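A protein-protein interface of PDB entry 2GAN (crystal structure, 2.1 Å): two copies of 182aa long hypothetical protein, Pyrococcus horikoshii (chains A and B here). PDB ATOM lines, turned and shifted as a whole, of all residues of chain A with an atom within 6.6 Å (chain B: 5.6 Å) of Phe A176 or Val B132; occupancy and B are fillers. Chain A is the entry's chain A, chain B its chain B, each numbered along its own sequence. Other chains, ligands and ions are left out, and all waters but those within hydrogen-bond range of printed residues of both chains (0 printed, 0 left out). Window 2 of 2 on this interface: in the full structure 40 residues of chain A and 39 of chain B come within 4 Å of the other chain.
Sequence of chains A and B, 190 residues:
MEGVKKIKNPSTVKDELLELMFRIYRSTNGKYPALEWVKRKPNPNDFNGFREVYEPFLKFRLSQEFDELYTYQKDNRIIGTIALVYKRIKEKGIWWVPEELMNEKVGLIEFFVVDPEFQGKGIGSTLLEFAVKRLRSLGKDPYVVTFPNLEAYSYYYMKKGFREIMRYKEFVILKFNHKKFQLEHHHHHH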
ATOM      1  N   LYS A 160     -36.915 -14.754  24.093  1.00  0.00           N
ATOM      2  CA  LYS A 160     -36.517 -15.177  25.427  1.00  0.00           C
ATOM      3  C   LYS A 160     -35.142 -14.620  25.788  1.00  0.00           C
ATOM      4  O   LYS A 160     -34.508 -15.071  26.743  1.00  0.00           O
ATOM      5  CB  LYS A 160     -36.488 -16.699  25.494  1.00  0.00           C
ATOM      6  CG  LYS A 160     -37.306 -17.278  26.619  1.00  0.00           C
ATOM      7  CD  LYS A 160     -38.762 -16.912  26.486  1.00  0.00           C
ATOM      8  CE  LYS A 160     -39.563 -17.533  27.606  1.00  0.00           C
ATOM      9  NZ  LYS A 160     -41.006 -17.197  27.499  1.00  0.00           N
ATOM     10  N   GLY A 161     -34.681 -13.651  25.003  1.00  0.00           N
ATOM     11  CA  GLY A 161     -33.396 -13.037  25.260  1.00  0.00           C
ATOM     12  C   GLY A 161     -32.283 -13.477  24.333  1.00  0.00           C
ATOM     13  O   GLY A 161     -31.179 -12.942  24.405  1.00  0.00           O
ATOM     14  N   PHE A 162     -32.551 -14.447  23.465  1.00  0.00           N
ATOM     15  CA  PHE A 162     -31.513 -14.916  22.555  1.00  0.00           C
ATOM     16  C   PHE A 162     -31.508 -14.149  21.236  1.00  0.00           C
ATOM     17  O   PHE A 162     -32.546 -13.677  20.775  1.00  0.00           O
ATOM     18  CB  PHE A 162     -31.663 -16.421  22.284  1.00  0.00           C
ATOM     19  CG  PHE A 162     -31.278 -17.300  23.452  1.00  0.00           C
ATOM     20  CD1 PHE A 162     -32.114 -17.428  24.557  1.00  0.00           C
ATOM     21  CD2 PHE A 162     -30.070 -17.991  23.448  1.00  0.00           C
ATOM     22  CE1 PHE A 162     -31.755 -18.235  25.643  1.00  0.00           C
ATOM     23  CE2 PHE A 162     -29.702 -18.799  24.526  1.00  0.00           C
ATOM     24  CZ  PHE A 162     -30.547 -18.919  25.627  1.00  0.00           C
ATOM     25  N   ARG A 163     -30.324 -14.012  20.645  1.00  0.00           N
ATOM     26  CA  ARG A 163     -30.160 -13.322  19.370  1.00  0.00           C
ATOM     27  C   ARG A 163     -29.321 -14.169  18.427  1.00  0.00           C
ATOM     28  O   ARG A 163     -28.459 -14.928  18.861  1.00  0.00           O
ATOM     29  CB  ARG A 163     -29.512 -11.948  19.571  1.00  0.00           C
ATOM     30  CG  ARG A 163     -30.511 -10.874  19.989  1.00  0.00           C
ATOM     31  CD  ARG A 163     -29.983  -9.453  19.758  1.00  0.00           C
ATOM     32  NE  ARG A 163     -31.057  -8.456  19.824  1.00  0.00           N
ATOM     33  CZ  ARG A 163     -32.090  -8.412  18.981  1.00  0.00           C
ATOM     34  NH1 ARG A 163     -33.020  -7.479  19.119  1.00  0.00           N
ATOM     35  NH2 ARG A 163     -32.188  -9.297  17.998  1.00  0.00           N
ATOM     36  N   ILE A 165     -26.458 -15.191  16.000  1.00  0.00           N
ATOM     37  CA  ILE A 165     -25.057 -14.796  15.898  1.00  0.00           C
ATOM     38  C   ILE A 165     -24.354 -15.523  14.761  1.00  0.00           C
ATOM     39  O   ILE A 165     -23.334 -15.059  14.256  1.00  0.00           O
ATOM     40  CB  ILE A 165     -24.292 -15.102  17.216  1.00  0.00           C
ATOM     41  CG1 ILE A 165     -24.989 -14.421  18.401  1.00  0.00           C
ATOM     42  CG2 ILE A 165     -22.846 -14.633  17.112  1.00  0.00           C
ATOM     43  CD1 ILE A 165     -25.129 -12.915  18.264  1.00  0.00           C
ATOM     44  N   LEU A 174     -27.622 -19.501  18.230  1.00  0.00           N
ATOM     45  CA  LEU A 174     -28.143 -18.314  18.907  1.00  0.00           C
ATOM     46  C   LEU A 174     -27.417 -18.131  20.236  1.00  0.00           C
ATOM     47  O   LEU A 174     -27.003 -19.106  20.866  1.00  0.00           O
ATOM     48  CB  LEU A 174     -29.641 -18.462  19.176  1.00  0.00           C
ATOM     49  CG  LEU A 174     -30.537 -18.887  18.012  1.00  0.00           C
ATOM     50  CD1 LEU A 174     -31.904 -19.263  18.548  1.00  0.00           C
ATOM     51  CD2 LEU A 174     -30.645 -17.762  16.995  1.00  0.00           C
ATOM     52  N   LYS A 175     -27.274 -16.883  20.662  1.00  0.00           N
ATOM     53  CA  LYS A 175     -26.589 -16.570  21.910  1.00  0.00           C
ATOM     54  C   LYS A 175     -27.452 -15.704  22.815  1.00  0.00           C
ATOM     55  O   LYS A 175     -28.078 -14.745  22.360  1.00  0.00           O
ATOM     56  CB  LYS A 175     -25.268 -15.845  21.624  1.00  0.00           C
ATOM     57  CG  LYS A 175     -24.538 -15.373  22.876  1.00  0.00           C
ATOM     58  CD  LYS A 175     -23.201 -14.712  22.551  1.00  0.00           C
ATOM     59  CE  LYS A 175     -22.514 -14.222  23.827  1.00  0.00           C
ATOM     60  NZ  LYS A 175     -21.164 -13.636  23.602  1.00  0.00           N
ATOM     61  N   PHE A 176     -27.487 -16.051  24.097  1.00  0.00           N
ATOM     62  CA  PHE A 176     -28.264 -15.294  25.068  1.00  0.00           C
ATOM     63  C   PHE A 176     -27.662 -13.913  25.280  1.00  0.00           C
ATOM     64  O   PHE A 176     -26.439 -13.754  25.283  1.00  0.00           O
ATOM     65  CB  PHE A 176     -28.295 -16.014  26.412  1.00  0.00           C
ATOM     66  CG  PHE A 176     -29.009 -15.252  27.486  1.00  0.00           C
ATOM     67  CD1 PHE A 176     -30.394 -15.146  27.478  1.00  0.00           C
ATOM     68  CD2 PHE A 176     -28.298 -14.620  28.498  1.00  0.00           C
ATOM     69  CE1 PHE A 176     -31.060 -14.420  28.468  1.00  0.00           C
ATOM     70  CE2 PHE A 176     -28.959 -13.893  29.491  1.00  0.00           C
ATOM     71  CZ  PHE A 176     -30.338 -13.792  29.474  1.00  0.00           C
ATOM     72  N   ASN A 177     -28.529 -12.923  25.463  1.00  0.00           N
ATOM     73  CA  ASN A 177     -28.108 -11.543  25.700  1.00  0.00           C
ATOM     74  C   ASN A 177     -28.791 -11.068  26.985  1.00  0.00           C
ATOM     75  O   ASN A 177     -30.018 -10.942  27.044  1.00  0.00           O
ATOM     76  CB  ASN A 177     -28.521 -10.652  24.522  1.00  0.00           C
ATOM     77  CG  ASN A 177     -27.780  -9.323  24.503  1.00  0.00           C
ATOM     78  OD1 ASN A 177     -26.575  -9.270  24.239  1.00  0.00           O
ATOM     79  ND2 ASN A 177     -28.497  -8.244  24.790  1.00  0.00           N
ATOM     80  N   HIS A 178     -27.988 -10.811  28.010  1.00  0.00           N
ATOM     81  CA  HIS A 178     -28.503 -10.381  29.309  1.00  0.00           C
ATOM     82  C   HIS A 178     -29.267  -9.059  29.277  1.00  0.00           C
ATOM     83  O   HIS A 178     -30.317  -8.931  29.904  1.00  0.00           O
ATOM     84  CB  HIS A 178     -27.351 -10.293  30.318  1.00  0.00           C
ATOM     85  CG  HIS A 178     -27.797 -10.075  31.730  1.00  0.00           C
ATOM     86  ND1 HIS A 178     -28.835 -10.781  32.299  1.00  0.00           N
ATOM     87  CD2 HIS A 178     -27.328  -9.252  32.696  1.00  0.00           C
ATOM     88  CE1 HIS A 178     -28.988 -10.400  33.556  1.00  0.00           C
ATOM     89  NE2 HIS A 178     -28.085  -9.473  33.821  1.00  0.00           N
ATOM     90  N   LYS A 179     -28.742  -8.077  28.552  1.00  0.00           N
ATOM     91  CA  LYS A 179     -29.397  -6.777  28.464  1.00  0.00           C
ATOM     92  C   LYS A 179     -30.656  -6.852  27.597  1.00  0.00           C
ATOM     93  O   LYS A 179     -31.600  -6.083  27.780  1.00  0.00           O
ATOM     94  CB  LYS A 179     -28.417  -5.732  27.917  1.00  0.00           C
ATOM     95  CG  LYS A 179     -27.876  -6.032  26.530  1.00  0.00           C
ATOM     96  CD  LYS A 179     -26.462  -5.484  26.343  1.00  0.00           C
ATOM     97  CE  LYS A 179     -26.342  -4.005  26.712  1.00  0.00           C
ATOM     98  NZ  LYS A 179     -27.173  -3.102  25.861  1.00  0.00           N
ATOM     99  N   LYS A 180     -30.667  -7.787  26.653  1.00  0.00           N
ATOM    100  CA  LYS A 180     -31.820  -7.972  25.781  1.00  0.00           C
ATOM    101  C   LYS A 180     -32.931  -8.655  26.577  1.00  0.00           C
ATOM    102  O   LYS A 180     -34.106  -8.302  26.462  1.00  0.00           O
ATOM    103  CB  LYS A 180     -31.424  -8.827  24.570  1.00  0.00           C
ATOM    104  CG  LYS A 180     -32.581  -9.518  23.857  1.00  0.00           C
ATOM    105  CD  LYS A 180     -33.615  -8.535  23.325  1.00  0.00           C
ATOM    106  CE  LYS A 180     -33.036  -7.631  22.243  1.00  0.00           C
ATOM    107  NZ  LYS A 180     -34.079  -6.748  21.643  1.00  0.00           N
ATOM    108  N   PHE A 181     -32.542  -9.630  27.392  1.00  0.00           N
ATOM    109  CA  PHE A 181     -33.481 -10.375  28.222  1.00  0.00           C
ATOM    110  C   PHE A 181     -34.250  -9.447  29.153  1.00  0.00           C
ATOM    111  O   PHE A 181     -35.478  -9.463  29.189  1.00  0.00           O
ATOM    112  CB  PHE A 181     -32.726 -11.414  29.053  1.00  0.00           C
ATOM    113  CG  PHE A 181     -33.608 -12.239  29.940  1.00  0.00           C
ATOM    114  CD1 PHE A 181     -34.485 -13.171  29.395  1.00  0.00           C
ATOM    115  CD2 PHE A 181     -33.560 -12.087  31.322  1.00  0.00           C
ATOM    116  CE1 PHE A 181     -35.303 -13.945  30.213  1.00  0.00           C
ATOM    117  CE2 PHE A 181     -34.372 -12.853  32.152  1.00  0.00           C
ATOM    118  CZ  PHE A 181     -35.245 -13.785  31.596  1.00  0.00           C
ATOM    119  N   GLN A 182     -33.514  -8.640  29.909  1.00  0.00           N
ATOM    120  CA  GLN A 182     -34.117  -7.709  30.851  1.00  0.00           C
ATOM    121  C   GLN A 182     -34.920  -6.630  30.134  1.00  0.00           C
ATOM    122  O   GLN A 182     -35.804  -6.007  30.722  1.00  0.00           O
ATOM    123  CB  GLN A 182     -33.032  -7.050  31.705  1.00  0.00           C
ATOM    124  CG  GLN A 182     -32.130  -8.035  32.423  1.00  0.00           C
ATOM    125  CD  GLN A 182     -31.175  -7.357  33.386  1.00  0.00           C
ATOM    126  OE1 GLN A 182     -31.594  -6.773  34.389  1.00  0.00           O
ATOM    127  NE2 GLN A 182     -29.882  -7.426  33.083  1.00  0.00           N
ATOM    128  N   ILE B 109     -26.798 -25.151  25.775  1.00  0.00           N
ATOM    129  CA  ILE B 109     -28.090 -25.556  26.306  1.00  0.00           C
ATOM    130  C   ILE B 109     -28.709 -26.448  25.236  1.00  0.00           C
ATOM    131  O   ILE B 109     -28.810 -26.049  24.080  1.00  0.00           O
ATOM    132  CB  ILE B 109     -29.007 -24.345  26.545  1.00  0.00           C
ATOM    133  CG1 ILE B 109     -28.482 -23.521  27.729  1.00  0.00           C
ATOM    134  CG2 ILE B 109     -30.442 -24.824  26.765  1.00  0.00           C
ATOM    135  CD1 ILE B 109     -29.324 -22.310  28.071  1.00  0.00           C
ATOM    136  N   LEU B 127     -37.460 -23.628  33.249  1.00  0.00           N
ATOM    137  CA  LEU B 127     -36.291 -24.431  32.912  1.00  0.00           C
ATOM    138  C   LEU B 127     -35.202 -23.633  32.211  1.00  0.00           C
ATOM    139  O   LEU B 127     -34.039 -23.698  32.596  1.00  0.00           O
ATOM    140  CB  LEU B 127     -36.703 -25.613  32.025  1.00  0.00           C
ATOM    141  CG  LEU B 127     -37.553 -26.711  32.679  1.00  0.00           C
ATOM    142  CD1 LEU B 127     -38.034 -27.682  31.615  1.00  0.00           C
ATOM    143  CD2 LEU B 127     -36.723 -27.449  33.742  1.00  0.00           C
ATOM    144  N   LEU B 128     -35.589 -22.882  31.185  1.00  0.00           N
ATOM    145  CA  LEU B 128     -34.647 -22.077  30.410  1.00  0.00           C
ATOM    146  C   LEU B 128     -33.985 -21.023  31.288  1.00  0.00           C
ATOM    147  O   LEU B 128     -32.764 -20.841  31.264  1.00  0.00           O
ATOM    148  CB  LEU B 128     -35.373 -21.392  29.247  1.00  0.00           C
ATOM    149  CG  LEU B 128     -34.462 -20.577  28.338  1.00  0.00           C
ATOM    150  CD1 LEU B 128     -33.381 -21.479  27.758  1.00  0.00           C
ATOM    151  CD2 LEU B 128     -35.284 -19.929  27.228  1.00  0.00           C
ATOM    152  N   GLU B 129     -34.804 -20.322  32.058  1.00  0.00           N
ATOM    153  CA  GLU B 129     -34.303 -19.294  32.956  1.00  0.00           C
ATOM    154  C   GLU B 129     -33.357 -19.945  33.968  1.00  0.00           C
ATOM    155  O   GLU B 129     -32.311 -19.394  34.295  1.00  0.00           O
ATOM    156  CB  GLU B 129     -35.467 -18.614  33.678  1.00  0.00           C
ATOM    157  CG  GLU B 129     -35.154 -17.192  34.096  1.00  0.00           C
ATOM    158  CD  GLU B 129     -36.383 -16.413  34.520  1.00  0.00           C
ATOM    159  OE1 GLU B 129     -37.412 -16.475  33.808  1.00  0.00           O
ATOM    160  OE2 GLU B 129     -36.307 -15.727  35.560  1.00  0.00           O
ATOM    161  N   PHE B 130     -33.713 -21.122  34.464  1.00  0.00           N
ATOM    162  CA  PHE B 130     -32.840 -21.788  35.412  1.00  0.00           C
ATOM    163  C   PHE B 130     -31.507 -22.075  34.722  1.00  0.00           C
ATOM    164  O   PHE B 130     -30.448 -21.695  35.213  1.00  0.00           O
ATOM    165  CB  PHE B 130     -33.463 -23.096  35.889  1.00  0.00           C
ATOM    166  CG  PHE B 130     -32.623 -23.835  36.892  1.00  0.00           C
ATOM    167  CD1 PHE B 130     -32.691 -23.522  38.249  1.00  0.00           C
ATOM    168  CD2 PHE B 130     -31.768 -24.851  36.482  1.00  0.00           C
ATOM    169  CE1 PHE B 130     -31.923 -24.217  39.184  1.00  0.00           C
ATOM    170  CE2 PHE B 130     -30.997 -25.552  37.402  1.00  0.00           C
ATOM    171  CZ  PHE B 130     -31.074 -25.237  38.756  1.00  0.00           C
ATOM    172  N   ALA B 131     -31.574 -22.744  33.574  1.00  0.00           N
ATOM    173  CA  ALA B 131     -30.388 -23.103  32.799  1.00  0.00           C
ATOM    174  C   ALA B 131     -29.499 -21.902  32.502  1.00  0.00           C
ATOM    175  O   ALA B 131     -28.282 -21.942  32.706  1.00  0.00           O
ATOM    176  CB  ALA B 131     -30.805 -23.761  31.492  1.00  0.00           C
ATOM    177  N   VAL B 132     -30.105 -20.834  32.010  1.00  0.00           N
ATOM    178  CA  VAL B 132     -29.348 -19.631  31.689  1.00  0.00           C
ATOM    179  C   VAL B 132     -28.600 -19.099  32.911  1.00  0.00           C
ATOM    180  O   VAL B 132     -27.432 -18.728  32.818  1.00  0.00           O
ATOM    181  CB  VAL B 132     -30.282 -18.517  31.156  1.00  0.00           C
ATOM    182  CG1 VAL B 132     -29.551 -17.179  31.146  1.00  0.00           C
ATOM    183  CG2 VAL B 132     -30.752 -18.871  29.754  1.00  0.00           C
ATOM    184  N   LYS B 133     -29.285 -19.063  34.049  1.00  0.00           N
ATOM    185  CA  LYS B 133     -28.707 -18.554  35.290  1.00  0.00           C
ATOM    186  C   LYS B 133     -27.537 -19.416  35.750  1.00  0.00           C
ATOM    187  O   LYS B 133     -26.453 -18.913  36.061  1.00  0.00           O
ATOM    188  CB  LYS B 133     -29.786 -18.514  36.370  1.00  0.00           C
ATOM    189  CG  LYS B 133     -29.427 -17.703  37.604  1.00  0.00           C
ATOM    190  CD  LYS B 133     -30.677 -17.385  38.431  1.00  0.00           C
ATOM    191  CE  LYS B 133     -31.690 -16.563  37.620  1.00  0.00           C
ATOM    192  NZ  LYS B 133     -32.972 -16.310  38.355  1.00  0.00           N
ATOM    193  N   ARG B 134     -27.768 -20.722  35.793  1.00  0.00           N
ATOM    194  CA  ARG B 134     -26.741 -21.662  36.205  1.00  0.00           C
ATOM    195  C   ARG B 134     -25.499 -21.484  35.323  1.00  0.00           C
ATOM    196  O   ARG B 134     -24.380 -21.390  35.822  1.00  0.00           O
ATOM    197  CB  ARG B 134     -27.310 -23.083  36.100  1.00  0.00           C
ATOM    198  CG  ARG B 134     -26.323 -24.207  36.290  1.00  0.00           C
ATOM    199  CD  ARG B 134     -25.735 -24.234  37.681  1.00  0.00           C
ATOM    200  NE  ARG B 134     -24.958 -25.451  37.891  1.00  0.00           N
ATOM    201  CZ  ARG B 134     -24.169 -25.659  38.940  1.00  0.00           C
ATOM    202  NH1 ARG B 134     -24.049 -24.720  39.875  1.00  0.00           N
ATOM    203  NH2 ARG B 134     -23.508 -26.806  39.064  1.00  0.00           N
ATOM    204  N   LEU B 135     -25.699 -21.415  34.011  1.00  0.00           N
ATOM    205  CA  LEU B 135     -24.575 -21.256  33.091  1.00  0.00           C
ATOM    206  C   LEU B 135     -23.797 -19.966  33.376  1.00  0.00           C
ATOM    207  O   LEU B 135     -22.568 -19.994  33.506  1.00  0.00           O
ATOM    208  CB  LEU B 135     -25.075 -21.288  31.640  1.00  0.00           C
ATOM    209  CG  LEU B 135     -24.644 -22.445  30.719  1.00  0.00           C
ATOM    210  CD1 LEU B 135     -24.342 -23.724  31.499  1.00  0.00           C
ATOM    211  CD2 LEU B 135     -25.744 -22.690  29.698  1.00  0.00           C
ATOM    212  N   ARG B 136     -24.507 -18.843  33.486  1.00  0.00           N
ATOM    213  CA  ARG B 136     -23.856 -17.561  33.773  1.00  0.00           C
ATOM    214  C   ARG B 136     -23.032 -17.639  35.064  1.00  0.00           C
ATOM    215  O   ARG B 136     -21.946 -17.066  35.155  1.00  0.00           O
ATOM    216  CB  ARG B 136     -24.902 -16.442  33.893  1.00  0.00           C
ATOM    217  CG  ARG B 136     -25.538 -16.044  32.570  1.00  0.00           C
ATOM    218  CD  ARG B 136     -26.763 -15.163  32.770  1.00  0.00           C
ATOM    219  NE  ARG B 136     -26.451 -13.872  33.379  1.00  0.00           N
ATOM    220  CZ  ARG B 136     -25.761 -12.904  32.779  1.00  0.00           C
ATOM    221  NH1 ARG B 136     -25.304 -13.077  31.543  1.00  0.00           N
ATOM    222  NH2 ARG B 136     -25.537 -11.757  33.408  1.00  0.00           N
ATOM    223  N   SER B 137     -23.547 -18.359  36.056  1.00  0.00           N
ATOM    224  CA  SER B 137     -22.848 -18.500  37.327  1.00  0.00           C
ATOM    225  C   SER B 137     -21.493 -19.162  37.115  1.00  0.00           C
ATOM    226  O   SER B 137     -20.482 -18.686  37.626  1.00  0.00           O
ATOM    227  CB  SER B 137     -23.687 -19.327  38.292  1.00  0.00           C
ATOM    228  OG  SER B 137     -24.967 -18.741  38.451  1.00  0.00           O
ATOM    229  N   LYS B 140     -20.132 -19.049  32.075  1.00  0.00           N
ATOM    230  CA  LYS B 140     -20.264 -19.512  30.703  1.00  0.00           C
ATOM    231  C   LYS B 140     -21.337 -18.707  29.982  1.00  0.00           C
ATOM    232  O   LYS B 140     -22.358 -18.356  30.571  1.00  0.00           O
ATOM    233  CB  LYS B 140     -20.641 -20.995  30.682  1.00  0.00           C
ATOM    234  CG  LYS B 140     -19.699 -21.905  31.462  1.00  0.00           C
ATOM    235  CD  LYS B 140     -18.382 -22.100  30.731  1.00  0.00           C
ATOM    236  CE  LYS B 140     -17.492 -23.112  31.439  1.00  0.00           C
ATOM    237  NZ  LYS B 140     -16.447 -23.644  30.518  1.00  0.00           N
ATOM    238  N   PRO B 142     -24.262 -18.717  27.583  1.00  0.00           N
ATOM    239  CA  PRO B 142     -25.194 -19.694  27.009  1.00  0.00           C
ATOM    240  C   PRO B 142     -25.471 -19.552  25.513  1.00  0.00           C
ATOM    241  O   PRO B 142     -25.721 -18.457  25.012  1.00  0.00           O
ATOM    242  CB  PRO B 142     -26.450 -19.524  27.871  1.00  0.00           C
ATOM    243  CG  PRO B 142     -26.393 -18.096  28.289  1.00  0.00           C
ATOM    244  CD  PRO B 142     -24.937 -17.843  28.563  1.00  0.00           C
ATOM    245  N   TYR B 143     -25.401 -20.682  24.814  1.00  0.00           N
ATOM    246  CA  TYR B 143     -25.655 -20.763  23.379  1.00  0.00           C
ATOM    247  C   TYR B 143     -26.594 -21.937  23.116  1.00  0.00           C
ATOM    248  O   TYR B 143     -26.601 -22.914  23.867  1.00  0.00           O
ATOM    249  CB  TYR B 143     -24.367 -21.030  22.590  1.00  0.00           C
ATOM    250  CG  TYR B 143     -23.415 -19.864  22.465  1.00  0.00           C
ATOM    251  CD1 TYR B 143     -22.481 -19.586  23.462  1.00  0.00           C
ATOM    252  CD2 TYR B 143     -23.453 -19.037  21.347  1.00  0.00           C
ATOM    253  CE1 TYR B 143     -21.605 -18.508  23.346  1.00  0.00           C
ATOM    254  CE2 TYR B 143     -22.586 -17.957  21.221  1.00  0.00           C
ATOM    255  CZ  TYR B 143     -21.667 -17.697  22.220  1.00  0.00           C
ATOM    256  OH  TYR B 143     -20.822 -16.618  22.098  1.00  0.00           O
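The side-chain amino group (NZ) of Lys A175 lies close to the side-chain hydroxyl (OH) of Tyr B143 (3.4 Å). N of Phe A176 is in hydrogen-bond range of O of Pro B142, 3.1 Å away. A ring nitrogen (NE2) of His A178 sits close to the guanidinium group (NH2) of Arg B136.
N of Ile B109 sits at hydrogen-bond distance from O of Tyr B143 (2.9 Å). The backbone carbonyl oxygen (O) of Arg A163 lies within hydrogen-bond range of the backbone NH (N) of Lys A175 (2.9 Å). The side-chain amide nitrogen (NE2) of Gln A182 lies within hydrogen-bond range of a ring nitrogen (NE2) of His A178, 2.8 Å away.
Among the printed residues, merely in contact across the chains: Lys A160 with Leu B128 (3.4 Å), Leu A174 with Tyr B143 (3.3 Å), Lys A175 with Pro B142 (3.7 Å) and Phe A176 with Val B132 (3.7 Å).
Ile A165 touches none of the printed residues of chain B. Printed residues of chain B within 4 Å of Leu A174: Tyr B143. Phe A176 touches just these residues of chain B: Val B132 and Pro B142. Printed residues of chain B within 4 Å of His A178: Arg B136. Val B132 touches just one residue of chain A: Phe A176. Printed residues of chain A within 4 Å of Arg B136: His A178 (3.2 Å). Of the printed residues of chain A, Pro B142 touches Lys A175 (3.7 Å) and Phe A176 (3.1 Å). Of the printed residues of chain A, Tyr B143 touches Leu A174 and Lys A175. The nearest residue of chain B that does not touch Phe A176 is Arg B136 (4.1 Å). The nearest residue of chain A that does not touch Val B132 is Phe A162 (4.1 Å).
Of the 15 printed residues of chain B, 5 touch a printed residue of chain A. Hydrophobic or aromatic side chains of chain B that line the printed part of chain A: Leu B128, Val B132, Pro B142 and Tyr B143. Of the 14 printed residues of chain A, 5 touch a printed residue of chain B. Printed residues of chain A that touch a printed residue of chain B: Lys A160, Leu A174, Lys A175, Phe A176 and His A178. Hydrophobic or aromatic side chains of chain A that line the printed part of chain B: Phe A176 and His A178. Along chain A the printed residues that touch a printed residue of chain B span positions 160 to 178. Among the printed residues, 7 pairs touch across the chains. Among the printed residues, no Asp or Glu carboxylate lies within 4 Å of a Lys or Arg side-chain nitrogen of the other chain.
No position is printed for both chains.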
